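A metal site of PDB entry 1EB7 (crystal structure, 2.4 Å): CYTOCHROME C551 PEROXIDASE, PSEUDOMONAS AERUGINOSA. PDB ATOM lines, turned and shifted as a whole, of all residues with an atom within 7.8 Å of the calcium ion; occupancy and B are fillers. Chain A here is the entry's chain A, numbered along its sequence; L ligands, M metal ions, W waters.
ND1 of His 261 lies within hydrogen-bond range of O4 of the ligand, at 2.6 Å.
The backbone NH (N) of Phe 260 lies within hydrogen-bond range of an oxygen (O2) of the ligand, at 2.7 Å.
An oxygen (O3) of the ligand sits at hydrogen-bond distance from the backbone NH (N) of His 261.
The backbone carbonyl oxygen (O) of Pro 66 is in hydrogen-bond range of the side-chain amide nitrogen (ND2) of Asn 79 (2.8 Å).
The backbone carbonyl oxygen of His 261 lies within hydrogen-bond range of the backbone NH of Asn 79, 2.7 Å away.
The side-chain amide nitrogen (ND2) of Asn 79 is in hydrogen-bond range of the backbone carbonyl oxygen (O) of Val 65, at 2.8 Å.
The backbone carbonyl oxygen of Asn 79 is in hydrogen-bond range of the indole nitrogen of Trp 94, at 2.8 Å.
Of the 20 residues printed, 3 come within 4 Å of the calcium ion.
The calcium ion is bound by OD1 of Asn 79, O of Thr 256, O of Pro 258, water W3, water W1, water W4 and water W2.
The calcium ion has seven donor atoms within binding distance.
Water W4 lies within hydrogen-bond range of OD1 of Asn 64 (3.1 Å), O of Ala 257 (3.2 Å) and ND2 of Asn 79 (3.4 Å).
Water W1 lies within hydrogen-bond range of the side-chain hydroxyl (OG1) of Thr 256 (2.8 Å) and an oxygen (O1) of the ligand (2.8 Å).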
ATOM      1  N   ALA A  62      -7.286 -19.890  -7.382  1.00  0.00           N
ATOM      2  CA  ALA A  62      -8.731 -19.738  -7.553  1.00  0.00           C
ATOM      3  C   ALA A  62      -8.980 -19.457  -9.040  1.00  0.00           C
ATOM      4  O   ALA A  62      -8.051 -19.066  -9.736  1.00  0.00           O
ATOM      5  CB  ALA A  62      -9.249 -18.596  -6.702  1.00  0.00           C
ATOM      6  N   ASP A  63     -10.201 -19.652  -9.526  1.00  0.00           N
ATOM      7  CA  ASP A  63     -10.472 -19.406 -10.937  1.00  0.00           C
ATOM      8  C   ASP A  63     -10.687 -17.929 -11.272  1.00  0.00           C
ATOM      9  O   ASP A  63     -10.673 -17.520 -12.423  1.00  0.00           O
ATOM     10  CB  ASP A  63     -11.640 -20.244 -11.460  1.00  0.00           C
ATOM     11  CG  ASP A  63     -12.895 -20.085 -10.651  1.00  0.00           C
ATOM     12  OD1 ASP A  63     -13.073 -19.036  -9.987  1.00  0.00           O
ATOM     13  OD2 ASP A  63     -13.728 -21.013 -10.671  1.00  0.00           O
ATOM     14  N   ASN A  64     -10.917 -17.130 -10.244  1.00  0.00           N
ATOM     15  CA  ASN A  64     -11.107 -15.706 -10.445  1.00  0.00           C
ATOM     16  C   ASN A  64     -12.234 -15.255 -11.372  1.00  0.00           C
ATOM     17  O   ASN A  64     -12.099 -14.292 -12.146  1.00  0.00           O
ATOM     18  CB  ASN A  64      -9.781 -15.054 -10.787  1.00  0.00           C
ATOM     19  CG  ASN A  64      -8.851 -15.084  -9.608  1.00  0.00           C
ATOM     20  OD1 ASN A  64      -9.303 -15.347  -8.478  1.00  0.00           O
ATOM     21  ND2 ASN A  64      -7.559 -14.872  -9.838  1.00  0.00           N
ATOM     22  N   VAL A  65     -13.331 -16.002 -11.353  1.00  0.00           N
ATOM     23  CA  VAL A  65     -14.520 -15.625 -12.082  1.00  0.00           C
ATOM     24  C   VAL A  65     -15.554 -15.504 -10.962  1.00  0.00           C
ATOM     25  O   VAL A  65     -15.415 -16.134  -9.907  1.00  0.00           O
ATOM     26  CB  VAL A  65     -14.915 -16.670 -13.130  1.00  0.00           C
ATOM     27  CG1 VAL A  65     -13.868 -16.714 -14.214  1.00  0.00           C
ATOM     28  CG2 VAL A  65     -15.092 -18.041 -12.499  1.00  0.00           C
ATOM     29  N   PRO A  66     -16.614 -14.696 -11.163  1.00  0.00           N
ATOM     30  CA  PRO A  66     -17.629 -14.529 -10.127  1.00  0.00           C
ATOM     31  C   PRO A  66     -18.047 -15.787  -9.367  1.00  0.00           C
ATOM     32  O   PRO A  66     -17.880 -15.869  -8.160  1.00  0.00           O
ATOM     33  CB  PRO A  66     -18.786 -13.890 -10.881  1.00  0.00           C
ATOM     34  CG  PRO A  66     -18.070 -13.010 -11.875  1.00  0.00           C
ATOM     35  CD  PRO A  66     -16.984 -13.959 -12.384  1.00  0.00           C
ATOM     36  N   ASN A  79     -18.252 -18.116  -5.260  1.00  0.00           N
ATOM     37  CA  ASN A  79     -16.942 -17.790  -5.776  1.00  0.00           C
ATOM     38  C   ASN A  79     -16.009 -18.887  -5.288  1.00  0.00           C
ATOM     39  O   ASN A  79     -16.092 -19.283  -4.127  1.00  0.00           O
ATOM     40  CB  ASN A  79     -16.489 -16.444  -5.224  1.00  0.00           C
ATOM     41  CG  ASN A  79     -15.232 -15.934  -5.874  1.00  0.00           C
ATOM     42  OD1 ASN A  79     -14.180 -15.715  -5.214  1.00  0.00           O
ATOM     43  ND2 ASN A  79     -15.310 -15.718  -7.185  1.00  0.00           N
ATOM     44  N   SER A  80     -15.181 -19.429  -6.174  1.00  0.00           N
ATOM     45  CA  SER A  80     -14.237 -20.469  -5.767  1.00  0.00           C
ATOM     46  C   SER A  80     -13.145 -19.878  -4.893  1.00  0.00           C
ATOM     47  O   SER A  80     -12.430 -18.937  -5.298  1.00  0.00           O
ATOM     48  CB  SER A  80     -13.565 -21.085  -6.982  1.00  0.00           C
ATOM     49  OG  SER A  80     -14.535 -21.495  -7.923  1.00  0.00           O
ATOM     50  N   PRO A  81     -13.014 -20.382  -3.656  1.00  0.00           N
ATOM     51  CA  PRO A  81     -11.995 -19.902  -2.732  1.00  0.00           C
ATOM     52  C   PRO A  81     -10.665 -20.521  -3.149  1.00  0.00           C
ATOM     53  O   PRO A  81     -10.660 -21.582  -3.799  1.00  0.00           O
ATOM     54  CB  PRO A  81     -12.453 -20.493  -1.404  1.00  0.00           C
ATOM     55  CG  PRO A  81     -12.997 -21.824  -1.836  1.00  0.00           C
ATOM     56  CD  PRO A  81     -13.829 -21.446  -3.038  1.00  0.00           C
ATOM     57  N   THR A  82      -9.551 -19.877  -2.798  1.00  0.00           N
ATOM     58  CA  THR A  82      -8.257 -20.408  -3.165  1.00  0.00           C
ATOM     59  C   THR A  82      -8.010 -21.709  -2.436  1.00  0.00           C
ATOM     60  O   THR A  82      -8.558 -21.932  -1.359  1.00  0.00           O
ATOM     61  CB  THR A  82      -7.117 -19.455  -2.790  1.00  0.00           C
ATOM     62  OG1 THR A  82      -5.867 -20.104  -3.042  1.00  0.00           O
ATOM     63  CG2 THR A  82      -7.189 -19.073  -1.336  1.00  0.00           C
ATOM     64  N   TRP A  94     -18.604 -21.694   2.294  1.00  0.00           N
ATOM     65  CA  TRP A  94     -19.067 -20.324   2.423  1.00  0.00           C
ATOM     66  C   TRP A  94     -20.191 -20.065   3.394  1.00  0.00           C
ATOM     67  O   TRP A  94     -20.093 -19.208   4.254  1.00  0.00           O
ATOM     68  CB  TRP A  94     -19.541 -19.792   1.075  1.00  0.00           C
ATOM     69  CG  TRP A  94     -18.478 -19.262   0.210  1.00  0.00           C
ATOM     70  CD1 TRP A  94     -18.058 -19.776  -0.988  1.00  0.00           C
ATOM     71  CD2 TRP A  94     -17.713 -18.067   0.442  1.00  0.00           C
ATOM     72  NE1 TRP A  94     -17.081 -18.969  -1.521  1.00  0.00           N
ATOM     73  CE2 TRP A  94     -16.847 -17.927  -0.679  1.00  0.00           C
ATOM     74  CE3 TRP A  94     -17.671 -17.121   1.462  1.00  0.00           C
ATOM     75  CZ2 TRP A  94     -15.965 -16.859  -0.794  1.00  0.00           C
ATOM     76  CZ3 TRP A  94     -16.788 -16.053   1.347  1.00  0.00           C
ATOM     77  CH2 TRP A  94     -15.943 -15.933   0.230  1.00  0.00           C
ATOM     78  N   VAL A 253      -5.263 -12.524  -0.493  1.00  0.00           N
ATOM     79  CA  VAL A 253      -6.478 -11.886  -0.970  1.00  0.00           C
ATOM     80  C   VAL A 253      -6.294 -10.939  -2.166  1.00  0.00           C
ATOM     81  O   VAL A 253      -7.207 -10.752  -2.969  1.00  0.00           O
ATOM     82  CB  VAL A 253      -7.185 -11.172   0.181  1.00  0.00           C
ATOM     83  CG1 VAL A 253      -6.300 -10.091   0.744  1.00  0.00           C
ATOM     84  CG2 VAL A 253      -8.527 -10.640  -0.261  1.00  0.00           C
ATOM     85  N   LEU A 255      -4.698 -11.493  -4.693  1.00  0.00           N
ATOM     86  CA  LEU A 255      -4.581 -12.311  -5.901  1.00  0.00           C
ATOM     87  C   LEU A 255      -5.858 -13.032  -6.309  1.00  0.00           C
ATOM     88  O   LEU A 255      -5.871 -13.675  -7.370  1.00  0.00           O
ATOM     89  CB  LEU A 255      -3.535 -13.411  -5.683  1.00  0.00           C
ATOM     90  CG  LEU A 255      -2.191 -13.012  -5.076  1.00  0.00           C
ATOM     91  CD1 LEU A 255      -1.255 -14.194  -5.128  1.00  0.00           C
ATOM     92  CD2 LEU A 255      -1.602 -11.822  -5.848  1.00  0.00           C
ATOM     93  N   THR A 256      -6.894 -12.967  -5.486  1.00  0.00           N
ATOM     94  CA  THR A 256      -8.121 -13.709  -5.785  1.00  0.00           C
ATOM     95  C   THR A 256      -9.440 -12.962  -5.941  1.00  0.00           C
ATOM     96  O   THR A 256     -10.517 -13.454  -5.506  1.00  0.00           O
ATOM     97  CB  THR A 256      -8.274 -14.834  -4.761  1.00  0.00           C
ATOM     98  OG1 THR A 256      -8.309 -14.250  -3.453  1.00  0.00           O
ATOM     99  CG2 THR A 256      -7.084 -15.797  -4.820  1.00  0.00           C
ATOM    100  N   ALA A 257      -9.395 -11.795  -6.577  1.00  0.00           N
ATOM    101  CA  ALA A 257     -10.616 -11.034  -6.832  1.00  0.00           C
ATOM    102  C   ALA A 257     -11.374 -11.837  -7.902  1.00  0.00           C
ATOM    103  O   ALA A 257     -10.773 -12.610  -8.644  1.00  0.00           O
ATOM    104  CB  ALA A 257     -10.270  -9.643  -7.340  1.00  0.00           C
ATOM    105  N   PRO A 258     -12.708 -11.700  -7.969  1.00  0.00           N
ATOM    106  CA  PRO A 258     -13.616 -10.884  -7.179  1.00  0.00           C
ATOM    107  C   PRO A 258     -13.824 -11.465  -5.773  1.00  0.00           C
ATOM    108  O   PRO A 258     -13.426 -12.626  -5.488  1.00  0.00           O
ATOM    109  CB  PRO A 258     -14.903 -10.907  -7.994  1.00  0.00           C
ATOM    110  CG  PRO A 258     -14.909 -12.307  -8.539  1.00  0.00           C
ATOM    111  CD  PRO A 258     -13.461 -12.521  -8.948  1.00  0.00           C
ATOM    112  N   TYR A 259     -14.492 -10.676  -4.937  1.00  0.00           N
ATOM    113  CA  TYR A 259     -14.705 -10.984  -3.544  1.00  0.00           C
ATOM    114  C   TYR A 259     -16.110 -11.341  -3.069  1.00  0.00           C
ATOM    115  O   TYR A 259     -17.100 -11.128  -3.775  1.00  0.00           O
ATOM    116  CB  TYR A 259     -14.164  -9.816  -2.733  1.00  0.00           C
ATOM    117  CG  TYR A 259     -12.747  -9.538  -3.116  1.00  0.00           C
ATOM    118  CD1 TYR A 259     -12.413  -8.416  -3.867  1.00  0.00           C
ATOM    119  CD2 TYR A 259     -11.727 -10.407  -2.754  1.00  0.00           C
ATOM    120  CE1 TYR A 259     -11.095  -8.181  -4.269  1.00  0.00           C
ATOM    121  CE2 TYR A 259     -10.414 -10.184  -3.135  1.00  0.00           C
ATOM    122  CZ  TYR A 259     -10.103  -9.081  -3.892  1.00  0.00           C
ATOM    123  OH  TYR A 259      -8.798  -8.905  -4.296  1.00  0.00           O
ATOM    124  N   PHE A 260     -16.173 -11.884  -1.855  1.00  0.00           N
ATOM    125  CA  PHE A 260     -17.407 -12.325  -1.205  1.00  0.00           C
ATOM    126  C   PHE A 260     -17.954 -13.562  -1.918  1.00  0.00           C
ATOM    127  O   PHE A 260     -17.593 -13.826  -3.054  1.00  0.00           O
ATOM    128  CB  PHE A 260     -18.397 -11.164  -1.119  1.00  0.00           C
ATOM    129  CG  PHE A 260     -17.868  -9.961  -0.353  1.00  0.00           C
ATOM    130  CD1 PHE A 260     -17.517  -8.788  -1.009  1.00  0.00           C
ATOM    131  CD2 PHE A 260     -17.674 -10.028   1.025  1.00  0.00           C
ATOM    132  CE1 PHE A 260     -16.988  -7.700  -0.307  1.00  0.00           C
ATOM    133  CE2 PHE A 260     -17.142  -8.941   1.737  1.00  0.00           C
ATOM    134  CZ  PHE A 260     -16.804  -7.777   1.073  1.00  0.00           C
ATOM    135  N   HIS A 261     -18.784 -14.329  -1.235  1.00  0.00           N
ATOM    136  CA  HIS A 261     -19.322 -15.582  -1.764  1.00  0.00           C
ATOM    137  C   HIS A 261     -19.942 -15.583  -3.136  1.00  0.00           C
ATOM    138  O   HIS A 261     -20.011 -16.628  -3.794  1.00  0.00           O
ATOM    139  CB  HIS A 261     -20.343 -16.164  -0.781  1.00  0.00           C
ATOM    140  CG  HIS A 261     -21.605 -15.379  -0.699  1.00  0.00           C
ATOM    141  ND1 HIS A 261     -21.695 -14.198   0.007  1.00  0.00           N
ATOM    142  CD2 HIS A 261     -22.829 -15.587  -1.268  1.00  0.00           C
ATOM    143  CE1 HIS A 261     -22.915 -13.698  -0.139  1.00  0.00           C
ATOM    144  NE2 HIS A 261     -23.619 -14.510  -0.902  1.00  0.00           N
ATOM    145  N   GLY A 263     -18.985 -13.352  -5.385  1.00  0.00           N
ATOM    146  CA  GLY A 263     -17.980 -12.808  -6.274  1.00  0.00           C
ATOM    147  C   GLY A 263     -18.477 -11.567  -6.962  1.00  0.00           C
ATOM    148  O   GLY A 263     -18.169 -11.334  -8.118  1.00  0.00           O
ATOM    149  N   VAL A 265     -17.960  -8.132  -5.844  1.00  0.00           N
ATOM    150  CA  VAL A 265     -17.162  -6.902  -5.795  1.00  0.00           C
ATOM    151  C   VAL A 265     -15.752  -7.220  -6.257  1.00  0.00           C
ATOM    152  O   VAL A 265     -15.100  -8.132  -5.756  1.00  0.00           O
ATOM    153  CB  VAL A 265     -17.214  -6.132  -4.422  1.00  0.00           C
ATOM    154  CG1 VAL A 265     -18.123  -6.810  -3.438  1.00  0.00           C
ATOM    155  CG2 VAL A 265     -15.820  -5.860  -3.883  1.00  0.00           C
HETATM  156 FE1  LIG L   1     -14.598  -9.576   6.768  1.00  0.00          FE
HETATM  157  C1  LIG L   1     -15.240 -11.338   4.017  1.00  0.00           C
HETATM  158  C2  LIG L   1     -12.287  -7.803   5.142  1.00  0.00           C
HETATM  159  C3  LIG L   1     -14.431  -7.506   9.387  1.00  0.00           C
HETATM  160  C4  LIG L   1     -16.740 -11.531   8.537  1.00  0.00           C
HETATM  161  N1  LIG L   1     -13.916  -9.519   4.960  1.00  0.00           N
HETATM  162  C5  LIG L   1     -14.296 -10.313   3.902  1.00  0.00           C
HETATM  163  C6  LIG L   1     -13.527 -10.009   2.678  1.00  0.00           C
HETATM  164  C7  LIG L   1     -12.674  -9.009   3.023  1.00  0.00           C
HETATM  165  C8  LIG L   1     -12.928  -8.733   4.433  1.00  0.00           C
HETATM  166  C9  LIG L   1     -11.646  -8.385   2.135  1.00  0.00           C
HETATM  167  C10 LIG L   1     -13.639 -10.720   1.305  1.00  0.00           C
HETATM  168  C11 LIG L   1     -12.543 -11.783   1.178  1.00  0.00           C
HETATM  169  C12 LIG L   1     -12.758 -12.736  -0.014  1.00  0.00           C
HETATM  170  O1  LIG L   1     -11.856 -13.554  -0.303  1.00  0.00           O
HETATM  171  O2  LIG L   1     -13.836 -12.674  -0.649  1.00  0.00           O
HETATM  172  N2  LIG L   1     -13.640  -8.000   7.130  1.00  0.00           N
HETATM  173  C13 LIG L   1     -12.668  -7.405   6.380  1.00  0.00           C
HETATM  174  C14 LIG L   1     -12.140  -6.222   7.030  1.00  0.00           C
HETATM  175  C15 LIG L   1     -12.795  -6.080   8.246  1.00  0.00           C
HETATM  176  C16 LIG L   1     -13.715  -7.209   8.272  1.00  0.00           C
HETATM  177  C17 LIG L   1     -11.045  -5.414   6.403  1.00  0.00           C
HETATM  178  C18 LIG L   1     -12.768  -4.999   9.347  1.00  0.00           C
HETATM  179  C19 LIG L   1     -12.412  -3.587   8.942  1.00  0.00           C
HETATM  180  N3  LIG L   1     -15.399  -9.544   8.554  1.00  0.00           N
HETATM  181  C20 LIG L   1     -15.209  -8.604   9.544  1.00  0.00           C
HETATM  182  C21 LIG L   1     -15.821  -8.981  10.821  1.00  0.00           C
HETATM  183  C22 LIG L   1     -16.445 -10.172  10.571  1.00  0.00           C
HETATM  184  C23 LIG L   1     -16.178 -10.480   9.175  1.00  0.00           C
HETATM  185  C24 LIG L   1     -15.630  -8.303  12.180  1.00  0.00           C
HETATM  186  C25 LIG L   1     -17.151 -11.090  11.528  1.00  0.00           C
HETATM  187  C26 LIG L   1     -18.577 -10.744  11.778  1.00  0.00           C
HETATM  188  N4  LIG L   1     -15.766 -11.059   6.389  1.00  0.00           N
HETATM  189  C27 LIG L   1     -16.650 -11.714   7.202  1.00  0.00           C
HETATM  190  C28 LIG L   1     -17.541 -12.600   6.483  1.00  0.00           C
HETATM  191  C29 LIG L   1     -17.185 -12.521   5.216  1.00  0.00           C
HETATM  192  C30 LIG L   1     -15.999 -11.636   5.165  1.00  0.00           C
HETATM  193  C31 LIG L   1     -18.728 -13.385   7.003  1.00  0.00           C
HETATM  194  C32 LIG L   1     -17.929 -13.144   4.025  1.00  0.00           C
HETATM  195  C33 LIG L   1     -19.201 -12.467   3.598  1.00  0.00           C
HETATM  196  C34 LIG L   1     -19.718 -12.990   2.282  1.00  0.00           C
HETATM  197  O3  LIG L   1     -19.002 -13.722   1.574  1.00  0.00           O
HETATM  198  O4  LIG L   1     -20.867 -12.657   1.923  1.00  0.00           O
HETATM  199 CA    CA M   1     -12.369 -14.489  -4.808  1.00  0.00          CA
HETATM  200  O   HOH W   1     -11.058 -13.951  -2.990  1.00  0.00           O
HETATM  201  O   HOH W   2     -13.641 -14.579  -2.842  1.00  0.00           O
HETATM  202  O   HOH W   3     -11.440 -16.477  -4.241  1.00  0.00           O
HETATM  203  O   HOH W   4     -11.993 -15.137  -7.008  1.00  0.00           O
